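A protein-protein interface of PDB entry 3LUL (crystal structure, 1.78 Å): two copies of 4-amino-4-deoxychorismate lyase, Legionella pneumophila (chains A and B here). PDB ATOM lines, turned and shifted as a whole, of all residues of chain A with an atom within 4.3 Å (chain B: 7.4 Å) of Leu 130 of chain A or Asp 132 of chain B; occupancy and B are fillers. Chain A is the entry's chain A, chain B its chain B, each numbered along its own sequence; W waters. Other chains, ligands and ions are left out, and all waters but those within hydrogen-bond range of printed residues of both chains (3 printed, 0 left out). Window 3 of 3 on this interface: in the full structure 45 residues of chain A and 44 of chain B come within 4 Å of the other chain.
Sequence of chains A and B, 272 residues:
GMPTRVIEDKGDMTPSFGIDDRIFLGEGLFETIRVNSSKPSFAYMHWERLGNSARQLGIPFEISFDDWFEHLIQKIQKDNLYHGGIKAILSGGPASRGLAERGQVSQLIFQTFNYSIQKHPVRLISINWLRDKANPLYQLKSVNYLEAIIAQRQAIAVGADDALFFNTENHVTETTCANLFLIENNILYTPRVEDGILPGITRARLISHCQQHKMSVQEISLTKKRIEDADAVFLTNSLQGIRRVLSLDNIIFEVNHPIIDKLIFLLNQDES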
ATOM      1  N   ASN A 128     -25.011 -13.398  -4.158  1.00  0.00           N
ATOM      2  CA  ASN A 128     -25.556 -12.051  -4.276  1.00  0.00           C
ATOM      3  C   ASN A 128     -24.543 -10.989  -4.705  1.00  0.00           C
ATOM      4  O   ASN A 128     -24.884 -10.062  -5.444  1.00  0.00           O
ATOM      5  CB  ASN A 128     -26.217 -11.641  -2.954  1.00  0.00           C
ATOM      6  CG  ASN A 128     -25.224 -11.404  -1.828  1.00  0.00           C
ATOM      7  OD1 ASN A 128     -24.473 -12.298  -1.464  1.00  0.00           O
ATOM      8  ND2 ASN A 128     -25.241 -10.185  -1.241  1.00  0.00           N
ATOM      9  N   TRP A 129     -23.303 -11.112  -4.269  1.00  0.00           N
ATOM     10  CA  TRP A 129     -22.308 -10.131  -4.688  1.00  0.00           C
ATOM     11  C   TRP A 129     -21.786 -10.446  -6.083  1.00  0.00           C
ATOM     12  O   TRP A 129     -21.676 -11.628  -6.511  1.00  0.00           O
ATOM     13  CB  TRP A 129     -21.182  -9.972  -3.652  1.00  0.00           C
ATOM     14  CG  TRP A 129     -20.249 -11.136  -3.537  1.00  0.00           C
ATOM     15  CD1 TRP A 129     -19.150 -11.346  -4.284  1.00  0.00           C
ATOM     16  CD2 TRP A 129     -20.285 -12.204  -2.577  1.00  0.00           C
ATOM     17  NE1 TRP A 129     -18.511 -12.491  -3.888  1.00  0.00           N
ATOM     18  CE2 TRP A 129     -19.185 -13.042  -2.846  1.00  0.00           C
ATOM     19  CE3 TRP A 129     -21.130 -12.529  -1.522  1.00  0.00           C
ATOM     20  CZ2 TRP A 129     -18.905 -14.199  -2.092  1.00  0.00           C
ATOM     21  CZ3 TRP A 129     -20.859 -13.664  -0.778  1.00  0.00           C
ATOM     22  CH2 TRP A 129     -19.762 -14.486  -1.059  1.00  0.00           C
ATOM     23  N   LEU A 130     -21.453  -9.384  -6.809  1.00  0.00           N
ATOM     24  CA  LEU A 130     -21.060  -9.474  -8.211  1.00  0.00           C
ATOM     25  C   LEU A 130     -19.564  -9.196  -8.389  1.00  0.00           C
ATOM     26  O   LEU A 130     -18.980  -8.485  -7.594  1.00  0.00           O
ATOM     27  CB  LEU A 130     -21.891  -8.471  -9.021  1.00  0.00           C
ATOM     28  CG  LEU A 130     -23.421  -8.626  -8.964  1.00  0.00           C
ATOM     29  CD1 LEU A 130     -24.118  -7.580  -9.852  1.00  0.00           C
ATOM     30  CD2 LEU A 130     -23.815 -10.038  -9.405  1.00  0.00           C
ATOM     31  N   ARG A 131     -18.963  -9.774  -9.435  1.00  0.00           N
ATOM     32  CA  ARG A 131     -17.566  -9.569  -9.811  1.00  0.00           C
ATOM     33  C   ARG A 131     -17.442  -8.714 -11.090  1.00  0.00           C
ATOM     34  O   ARG A 131     -18.174  -8.902 -12.033  1.00  0.00           O
ATOM     35  CB  ARG A 131     -16.915 -10.911 -10.092  1.00  0.00           C
ATOM     36  CG  ARG A 131     -16.932 -11.809  -8.877  1.00  0.00           C
ATOM     37  CD  ARG A 131     -16.569 -13.221  -9.210  1.00  0.00           C
ATOM     38  NE  ARG A 131     -16.284 -13.978  -7.981  1.00  0.00           N
ATOM     39  CZ  ARG A 131     -15.874 -15.251  -8.011  1.00  0.00           C
ATOM     40  NH1 ARG A 131     -15.747 -15.895  -9.174  1.00  0.00           N
ATOM     41  NH2 ARG A 131     -15.586 -15.884  -6.875  1.00  0.00           N
ATOM     42  N   PHE A 166     -21.934 -14.409 -10.551  1.00  0.00           N
ATOM     43  CA  PHE A 166     -22.314 -13.529 -11.643  1.00  0.00           C
ATOM     44  C   PHE A 166     -21.407 -12.323 -11.644  1.00  0.00           C
ATOM     45  O   PHE A 166     -20.889 -11.924 -10.587  1.00  0.00           O
ATOM     46  CB  PHE A 166     -23.758 -13.060 -11.472  1.00  0.00           C
ATOM     47  CG  PHE A 166     -24.742 -14.162 -11.694  1.00  0.00           C
ATOM     48  CD1 PHE A 166     -24.950 -15.111 -10.717  1.00  0.00           C
ATOM     49  CD2 PHE A 166     -25.406 -14.299 -12.932  1.00  0.00           C
ATOM     50  CE1 PHE A 166     -25.860 -16.166 -10.910  1.00  0.00           C
ATOM     51  CE2 PHE A 166     -26.316 -15.382 -13.153  1.00  0.00           C
ATOM     52  CZ  PHE A 166     -26.530 -16.297 -12.169  1.00  0.00           C
ATOM     53  N   ASN A 167     -21.251 -11.738 -12.819  1.00  0.00           N
ATOM     54  CA  ASN A 167     -20.477 -10.522 -12.976  1.00  0.00           C
ATOM     55  C   ASN A 167     -21.339  -9.268 -12.851  1.00  0.00           C
ATOM     56  O   ASN A 167     -22.563  -9.341 -12.706  1.00  0.00           O
ATOM     57  CB  ASN A 167     -19.557 -10.576 -14.212  1.00  0.00           C
ATOM     58  CG  ASN A 167     -20.262 -10.417 -15.551  1.00  0.00           C
ATOM     59  OD1 ASN A 167     -21.361  -9.889 -15.637  1.00  0.00           O
ATOM     60  ND2 ASN A 167     -19.561 -10.772 -16.611  1.00  0.00           N
ATOM     61  N   THR A 168     -20.689  -8.095 -12.873  1.00  0.00           N
ATOM     62  CA  THR A 168     -21.403  -6.828 -12.711  1.00  0.00           C
ATOM     63  C   THR A 168     -22.237  -6.422 -13.936  1.00  0.00           C
ATOM     64  O   THR A 168     -22.944  -5.449 -13.899  1.00  0.00           O
ATOM     65  CB  THR A 168     -20.440  -5.684 -12.351  1.00  0.00           C
ATOM     66  OG1 THR A 168     -19.413  -5.567 -13.358  1.00  0.00           O
ATOM     67  CG2 THR A 168     -19.837  -5.922 -10.949  1.00  0.00           C
ATOM     68  N   ASN A 170     -24.401  -8.639 -14.860  1.00  0.00           N
ATOM     69  CA  ASN A 170     -25.409  -9.687 -14.591  1.00  0.00           C
ATOM     70  C   ASN A 170     -25.333 -10.922 -15.507  1.00  0.00           C
ATOM     71  O   ASN A 170     -26.344 -11.518 -15.848  1.00  0.00           O
ATOM     72  CB  ASN A 170     -26.801  -9.098 -14.571  1.00  0.00           C
ATOM     73  CG  ASN A 170     -26.892  -7.897 -13.641  1.00  0.00           C
ATOM     74  OD1 ASN A 170     -27.195  -6.798 -14.077  1.00  0.00           O
ATOM     75  ND2 ASN A 170     -26.580  -8.110 -12.370  1.00  0.00           N
ATOM     76  N   LEU B 130     -14.139  -2.405 -10.707  1.00  0.00           N
ATOM     77  CA  LEU B 130     -14.938  -1.999  -9.546  1.00  0.00           C
ATOM     78  C   LEU B 130     -15.201  -3.154  -8.580  1.00  0.00           C
ATOM     79  O   LEU B 130     -15.220  -4.309  -8.985  1.00  0.00           O
ATOM     80  CB  LEU B 130     -16.240  -1.375 -10.011  1.00  0.00           C
ATOM     81  CG  LEU B 130     -16.107  -0.208 -11.029  1.00  0.00           C
ATOM     82  CD1 LEU B 130     -17.521   0.310 -11.455  1.00  0.00           C
ATOM     83  CD2 LEU B 130     -15.253   0.951 -10.538  1.00  0.00           C
ATOM     84  N   ARG B 131     -15.455  -2.811  -7.320  1.00  0.00           N
ATOM     85  CA  ARG B 131     -15.775  -3.770  -6.257  1.00  0.00           C
ATOM     86  C   ARG B 131     -17.236  -3.654  -5.859  1.00  0.00           C
ATOM     87  O   ARG B 131     -17.756  -2.561  -5.690  1.00  0.00           O
ATOM     88  CB  ARG B 131     -14.914  -3.534  -5.014  1.00  0.00           C
ATOM     89  CG  ARG B 131     -13.461  -3.766  -5.239  1.00  0.00           C
ATOM     90  CD  ARG B 131     -12.569  -3.289  -4.072  1.00  0.00           C
ATOM     91  NE  ARG B 131     -11.202  -3.750  -4.308  1.00  0.00           N
ATOM     92  CZ  ARG B 131     -10.199  -3.516  -3.459  1.00  0.00           C
ATOM     93  NH1 ARG B 131     -10.417  -2.817  -2.356  1.00  0.00           N
ATOM     94  NH2 ARG B 131      -8.988  -3.989  -3.711  1.00  0.00           N
ATOM     95  N   ASP B 132     -17.897  -4.789  -5.676  1.00  0.00           N
ATOM     96  CA  ASP B 132     -19.239  -4.803  -5.091  1.00  0.00           C
ATOM     97  C   ASP B 132     -19.093  -4.584  -3.598  1.00  0.00           C
ATOM     98  O   ASP B 132     -18.437  -5.341  -2.909  1.00  0.00           O
ATOM     99  CB  ASP B 132     -19.940  -6.142  -5.352  1.00  0.00           C
ATOM    100  CG  ASP B 132     -21.437  -6.082  -5.119  1.00  0.00           C
ATOM    101  OD1 ASP B 132     -21.877  -5.261  -4.296  1.00  0.00           O
ATOM    102  OD2 ASP B 132     -22.175  -6.857  -5.761  1.00  0.00           O
ATOM    103  N   LYS B 133     -19.747  -3.547  -3.077  1.00  0.00           N
ATOM    104  CA  LYS B 133     -19.734  -3.293  -1.641  1.00  0.00           C
ATOM    105  C   LYS B 133     -20.308  -4.480  -0.822  1.00  0.00           C
ATOM    106  O   LYS B 133     -20.026  -4.623   0.374  1.00  0.00           O
ATOM    107  CB  LYS B 133     -20.535  -1.997  -1.351  1.00  0.00           C
ATOM    108  CG  LYS B 133     -22.032  -2.155  -1.483  1.00  0.00           C
ATOM    109  CD  LYS B 133     -22.758  -0.812  -1.278  1.00  0.00           C
ATOM    110  CE  LYS B 133     -24.256  -1.021  -1.169  1.00  0.00           C
ATOM    111  NZ  LYS B 133     -24.965   0.251  -1.481  1.00  0.00           N
ATOM    112  N   ALA B 134     -21.059  -5.367  -1.482  1.00  0.00           N
ATOM    113  CA  ALA B 134     -21.630  -6.566  -0.846  1.00  0.00           C
ATOM    114  C   ALA B 134     -20.672  -7.758  -0.764  1.00  0.00           C
ATOM    115  O   ALA B 134     -21.012  -8.781  -0.171  1.00  0.00           O
ATOM    116  CB  ALA B 134     -22.940  -6.968  -1.553  1.00  0.00           C
ATOM    117  N   ASN B 135     -19.479  -7.658  -1.369  1.00  0.00           N
ATOM    118  CA  ASN B 135     -18.505  -8.729  -1.359  1.00  0.00           C
ATOM    119  C   ASN B 135     -17.806  -8.685   0.008  1.00  0.00           C
ATOM    120  O   ASN B 135     -17.114  -7.724   0.321  1.00  0.00           O
ATOM    121  CB  ASN B 135     -17.497  -8.531  -2.504  1.00  0.00           C
ATOM    122  CG  ASN B 135     -16.515  -9.619  -2.625  1.00  0.00           C
ATOM    123  OD1 ASN B 135     -16.227 -10.326  -1.680  1.00  0.00           O
ATOM    124  ND2 ASN B 135     -15.968  -9.771  -3.837  1.00  0.00           N
ATOM    125  N   PRO B 136     -17.981  -9.729   0.804  1.00  0.00           N
ATOM    126  CA  PRO B 136     -17.473  -9.662   2.182  1.00  0.00           C
ATOM    127  C   PRO B 136     -15.943  -9.606   2.304  1.00  0.00           C
ATOM    128  O   PRO B 136     -15.403  -9.220   3.349  1.00  0.00           O
ATOM    129  CB  PRO B 136     -18.033 -10.938   2.820  1.00  0.00           C
ATOM    130  CG  PRO B 136     -18.324 -11.866   1.669  1.00  0.00           C
ATOM    131  CD  PRO B 136     -18.659 -11.013   0.512  1.00  0.00           C
ATOM    132  N   LEU B 137     -15.231  -9.982   1.243  1.00  0.00           N
ATOM    133  CA  LEU B 137     -13.784  -9.952   1.261  1.00  0.00           C
ATOM    134  C   LEU B 137     -13.230  -8.590   1.631  1.00  0.00           C
ATOM    135  O   LEU B 137     -12.203  -8.506   2.320  1.00  0.00           O
ATOM    136  CB  LEU B 137     -13.159 -10.421  -0.069  1.00  0.00           C
ATOM    137  CG  LEU B 137     -12.646 -11.849  -0.052  1.00  0.00           C
ATOM    138  CD1 LEU B 137     -11.377 -11.919   0.790  1.00  0.00           C
ATOM    139  CD2 LEU B 137     -13.762 -12.803   0.475  1.00  0.00           C
ATOM    140  N   TYR B 138     -13.920  -7.526   1.221  1.00  0.00           N
ATOM    141  CA  TYR B 138     -13.346  -6.180   1.323  1.00  0.00           C
ATOM    142  C   TYR B 138     -13.474  -5.574   2.727  1.00  0.00           C
ATOM    143  O   TYR B 138     -12.912  -4.523   2.998  1.00  0.00           O
ATOM    144  CB  TYR B 138     -13.905  -5.270   0.227  1.00  0.00           C
ATOM    145  CG  TYR B 138     -13.547  -5.779  -1.150  1.00  0.00           C
ATOM    146  CD1 TYR B 138     -12.192  -5.979  -1.528  1.00  0.00           C
ATOM    147  CD2 TYR B 138     -14.533  -6.105  -2.068  1.00  0.00           C
ATOM    148  CE1 TYR B 138     -11.859  -6.461  -2.767  1.00  0.00           C
ATOM    149  CE2 TYR B 138     -14.206  -6.613  -3.324  1.00  0.00           C
ATOM    150  CZ  TYR B 138     -12.861  -6.776  -3.665  1.00  0.00           C
ATOM    151  OH  TYR B 138     -12.540  -7.260  -4.892  1.00  0.00           O
ATOM    152  N   GLN B 139     -14.144  -6.265   3.638  1.00  0.00           N
ATOM    153  CA  GLN B 139     -14.193  -5.829   5.037  1.00  0.00           C
ATOM    154  C   GLN B 139     -13.362  -6.714   5.944  1.00  0.00           C
ATOM    155  O   GLN B 139     -13.378  -6.549   7.162  1.00  0.00           O
ATOM    156  CB  GLN B 139     -15.659  -5.765   5.494  1.00  0.00           C
ATOM    157  CG  GLN B 139     -16.449  -4.831   4.598  1.00  0.00           C
ATOM    158  CD  GLN B 139     -17.901  -4.631   5.032  1.00  0.00           C
ATOM    159  OE1 GLN B 139     -18.191  -4.371   6.208  1.00  0.00           O
ATOM    160  NE2 GLN B 139     -18.815  -4.697   4.065  1.00  0.00           N
ATOM    161  N   PHE B 166     -12.673   1.967  -6.357  1.00  0.00           N
ATOM    162  CA  PHE B 166     -14.049   2.383  -6.360  1.00  0.00           C
ATOM    163  C   PHE B 166     -15.010   1.169  -6.347  1.00  0.00           C
ATOM    164  O   PHE B 166     -14.654   0.049  -6.795  1.00  0.00           O
ATOM    165  CB  PHE B 166     -14.301   3.245  -7.575  1.00  0.00           C
ATOM    166  CG  PHE B 166     -13.568   4.582  -7.538  1.00  0.00           C
ATOM    167  CD1 PHE B 166     -12.206   4.654  -7.809  1.00  0.00           C
ATOM    168  CD2 PHE B 166     -14.246   5.754  -7.218  1.00  0.00           C
ATOM    169  CE1 PHE B 166     -11.516   5.903  -7.731  1.00  0.00           C
ATOM    170  CE2 PHE B 166     -13.560   6.981  -7.158  1.00  0.00           C
ATOM    171  CZ  PHE B 166     -12.214   7.041  -7.422  1.00  0.00           C
ATOM    172  N   ASN B 167     -16.197   1.382  -5.785  1.00  0.00           N
ATOM    173  CA  ASN B 167     -17.224   0.350  -5.782  1.00  0.00           C
ATOM    174  C   ASN B 167     -18.091   0.469  -7.044  1.00  0.00           C
ATOM    175  O   ASN B 167     -17.892   1.386  -7.862  1.00  0.00           O
ATOM    176  CB  ASN B 167     -18.043   0.279  -4.463  1.00  0.00           C
ATOM    177  CG  ASN B 167     -18.922   1.485  -4.209  1.00  0.00           C
ATOM    178  OD1 ASN B 167     -19.322   2.190  -5.129  1.00  0.00           O
ATOM    179  ND2 ASN B 167     -19.272   1.691  -2.932  1.00  0.00           N
ATOM    180  N   THR B 168     -19.013  -0.480  -7.217  1.00  0.00           N
ATOM    181  CA  THR B 168     -19.875  -0.525  -8.398  1.00  0.00           C
ATOM    182  C   THR B 168     -20.964   0.558  -8.421  1.00  0.00           C
ATOM    183  O   THR B 168     -21.676   0.707  -9.420  1.00  0.00           O
ATOM    184  CB  THR B 168     -20.487  -1.957  -8.596  1.00  0.00           C
ATOM    185  OG1 THR B 168     -21.237  -2.301  -7.431  1.00  0.00           O
ATOM    186  CG2 THR B 168     -19.380  -3.010  -8.837  1.00  0.00           C
ATOM    187  N   GLU B 169     -21.043   1.372  -7.361  1.00  0.00           N
ATOM    188  CA  GLU B 169     -21.873   2.579  -7.353  1.00  0.00           C
ATOM    189  C   GLU B 169     -21.019   3.820  -7.655  1.00  0.00           C
ATOM    190  O   GLU B 169     -21.487   4.925  -7.483  1.00  0.00           O
ATOM    191  CB  GLU B 169     -22.591   2.718  -5.996  1.00  0.00           C
ATOM    192  CG  GLU B 169     -23.571   1.552  -5.724  1.00  0.00           C
ATOM    193  CD  GLU B 169     -24.072   1.490  -4.281  1.00  0.00           C
ATOM    194  OE1 GLU B 169     -23.572   2.242  -3.417  1.00  0.00           O
ATOM    195  OE2 GLU B 169     -24.967   0.668  -3.989  1.00  0.00           O
ATOM    196  N   THR B 173     -13.594   3.841  -2.216  1.00  0.00           N
ATOM    197  CA  THR B 173     -13.472   2.983  -1.033  1.00  0.00           C
ATOM    198  C   THR B 173     -12.144   3.294  -0.306  1.00  0.00           C
ATOM    199  O   THR B 173     -12.131   4.062   0.648  1.00  0.00           O
ATOM    200  CB  THR B 173     -13.676   1.488  -1.348  1.00  0.00           C
ATOM    201  OG1 THR B 173     -12.677   0.987  -2.278  1.00  0.00           O
ATOM    202  CG2 THR B 173     -15.060   1.316  -1.921  1.00  0.00           C
ATOM    203  N   ASP B 195     -19.860   1.545   2.284  1.00  0.00           N
ATOM    204  CA  ASP B 195     -19.361   1.631   0.922  1.00  0.00           C
ATOM    205  C   ASP B 195     -18.464   0.440   0.533  1.00  0.00           C
ATOM    206  O   ASP B 195     -18.066   0.328  -0.638  1.00  0.00           O
ATOM    207  CB  ASP B 195     -18.600   2.947   0.658  1.00  0.00           C
ATOM    208  CG  ASP B 195     -19.469   4.178   0.765  1.00  0.00           C
ATOM    209  OD1 ASP B 195     -20.668   4.096   0.397  1.00  0.00           O
ATOM    210  OD2 ASP B 195     -18.923   5.237   1.215  1.00  0.00           O
ATOM    211  N   GLY B 196     -18.136  -0.429   1.501  1.00  0.00           N
ATOM    212  CA  GLY B 196     -17.382  -1.639   1.268  1.00  0.00           C
ATOM    213  C   GLY B 196     -15.886  -1.475   1.489  1.00  0.00           C
ATOM    214  O   GLY B 196     -15.072  -1.774   0.613  1.00  0.00           O
HETATM  215  O   HOH W   1     -23.130  -9.868   0.792  1.00  0.00           O
HETATM  216  O   HOH W   2     -16.929  -7.538  -6.002  1.00  0.00           O
HETATM  217  O   HOH W   3     -24.772  -7.097  -5.447  1.00  0.00           O
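Water W1 lies within hydrogen-bond range of the backbone carbonyl oxygen of Ala 134 of chain B (2.6 Å) and the side-chain amide nitrogen of Asn 128 of chain A (2.9 Å).
Water W3 lies within hydrogen-bond range of OD2 of Asp 132 of chain B and O of Asn 128 of chain A.
Water W2 lies within hydrogen-bond range of O of Leu 130 of chain A, N of Asp 132 of chain B and ND2 of Asn 135 of chain B.
The backbone carbonyl oxygen of Arg 131 of chain A is in hydrogen-bond range of the backbone NH of Thr 168 of chain A (2.8 Å).
The backbone NH of Thr 168 of chain B lies within hydrogen-bond range of the backbone carbonyl oxygen of Arg 131 of chain B (2.9 Å).
OD1 of Asp 132 of chain B lies within hydrogen-bond range of N of Ala 134 of chain B (2.9 Å).
The side-chain amide oxygen (OD1) of Asn 135 of chain B lies within hydrogen-bond range of the backbone NH (N) of Leu 137 of chain B, 3.1 Å away.
Among the printed residues, merely in contact across the chains: Asn 128 of chain A with Ala 134 of chain B (3.97 Å), Trp 129 of chain A with Asp 132 of chain B (3.4 Å), Trp 129 of chain A with Ala 134 of chain B (3.7 Å), Trp 129 of chain A with Asn 135 of chain B (3.6 Å), Trp 129 of chain A with Pro 136 of chain B (3.5 Å) and Thr 168 of chain A with Thr 168 of chain B (3.6 Å).
Hydrophobic or aromatic side chains of chain A that line the printed part of chain B: Trp 129 and Leu 130.
Along chain A the printed residues that touch a printed residue of chain B span positions 128 to 168.
Among the printed residues, no Asp or Glu carboxylate lies within 4 Å of a Lys or Arg side-chain nitrogen of the other chain.
Thr 168 of chain B touches its own counterpart, Thr 168 of chain A.
5 positions are printed for both chains.
Of the 7 pairs that touch across the chains among the printed residues, 1 has its exchanged pair printed and touching as well.
OD2 of Asp 132 of chain B lies within hydrogen-bond range of N of Leu 130 of chain A (2.8 Å).
Leu 130 of chain A touches one residue of chain B.
Asp 132 of chain B touches just these residues of chain A: Trp 129 (3.4 Å) and Leu 130 (2.8 Å).
Of the printed residues of chain A, Pro 136 of chain B touches Trp 129 (3.5 Å).
Of the printed residues of chain B, Thr 168 of chain A touches Thr 168 (3.6 Å).
Of the printed residues of chain A, Thr 168 of chain B touches Thr 168.
Of the printed residues of chain B, Asn 128 of chain A touches Ala 134 (3.97 Å).
Asn 167 of chain B touches none of the printed residues of chain A.
The nearest residue of chain B that does not touch Leu 130 of chain A is Asn 135 of chain B (5.0 Å).
The nearest residue of chain A that does not touch Asp 132 of chain B is Asn 128 of chain A (4.2 Å).
The nearest printed residue of chain B that does not touch Asn 128 of chain A is Asp 132 of chain B (4.2 Å).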
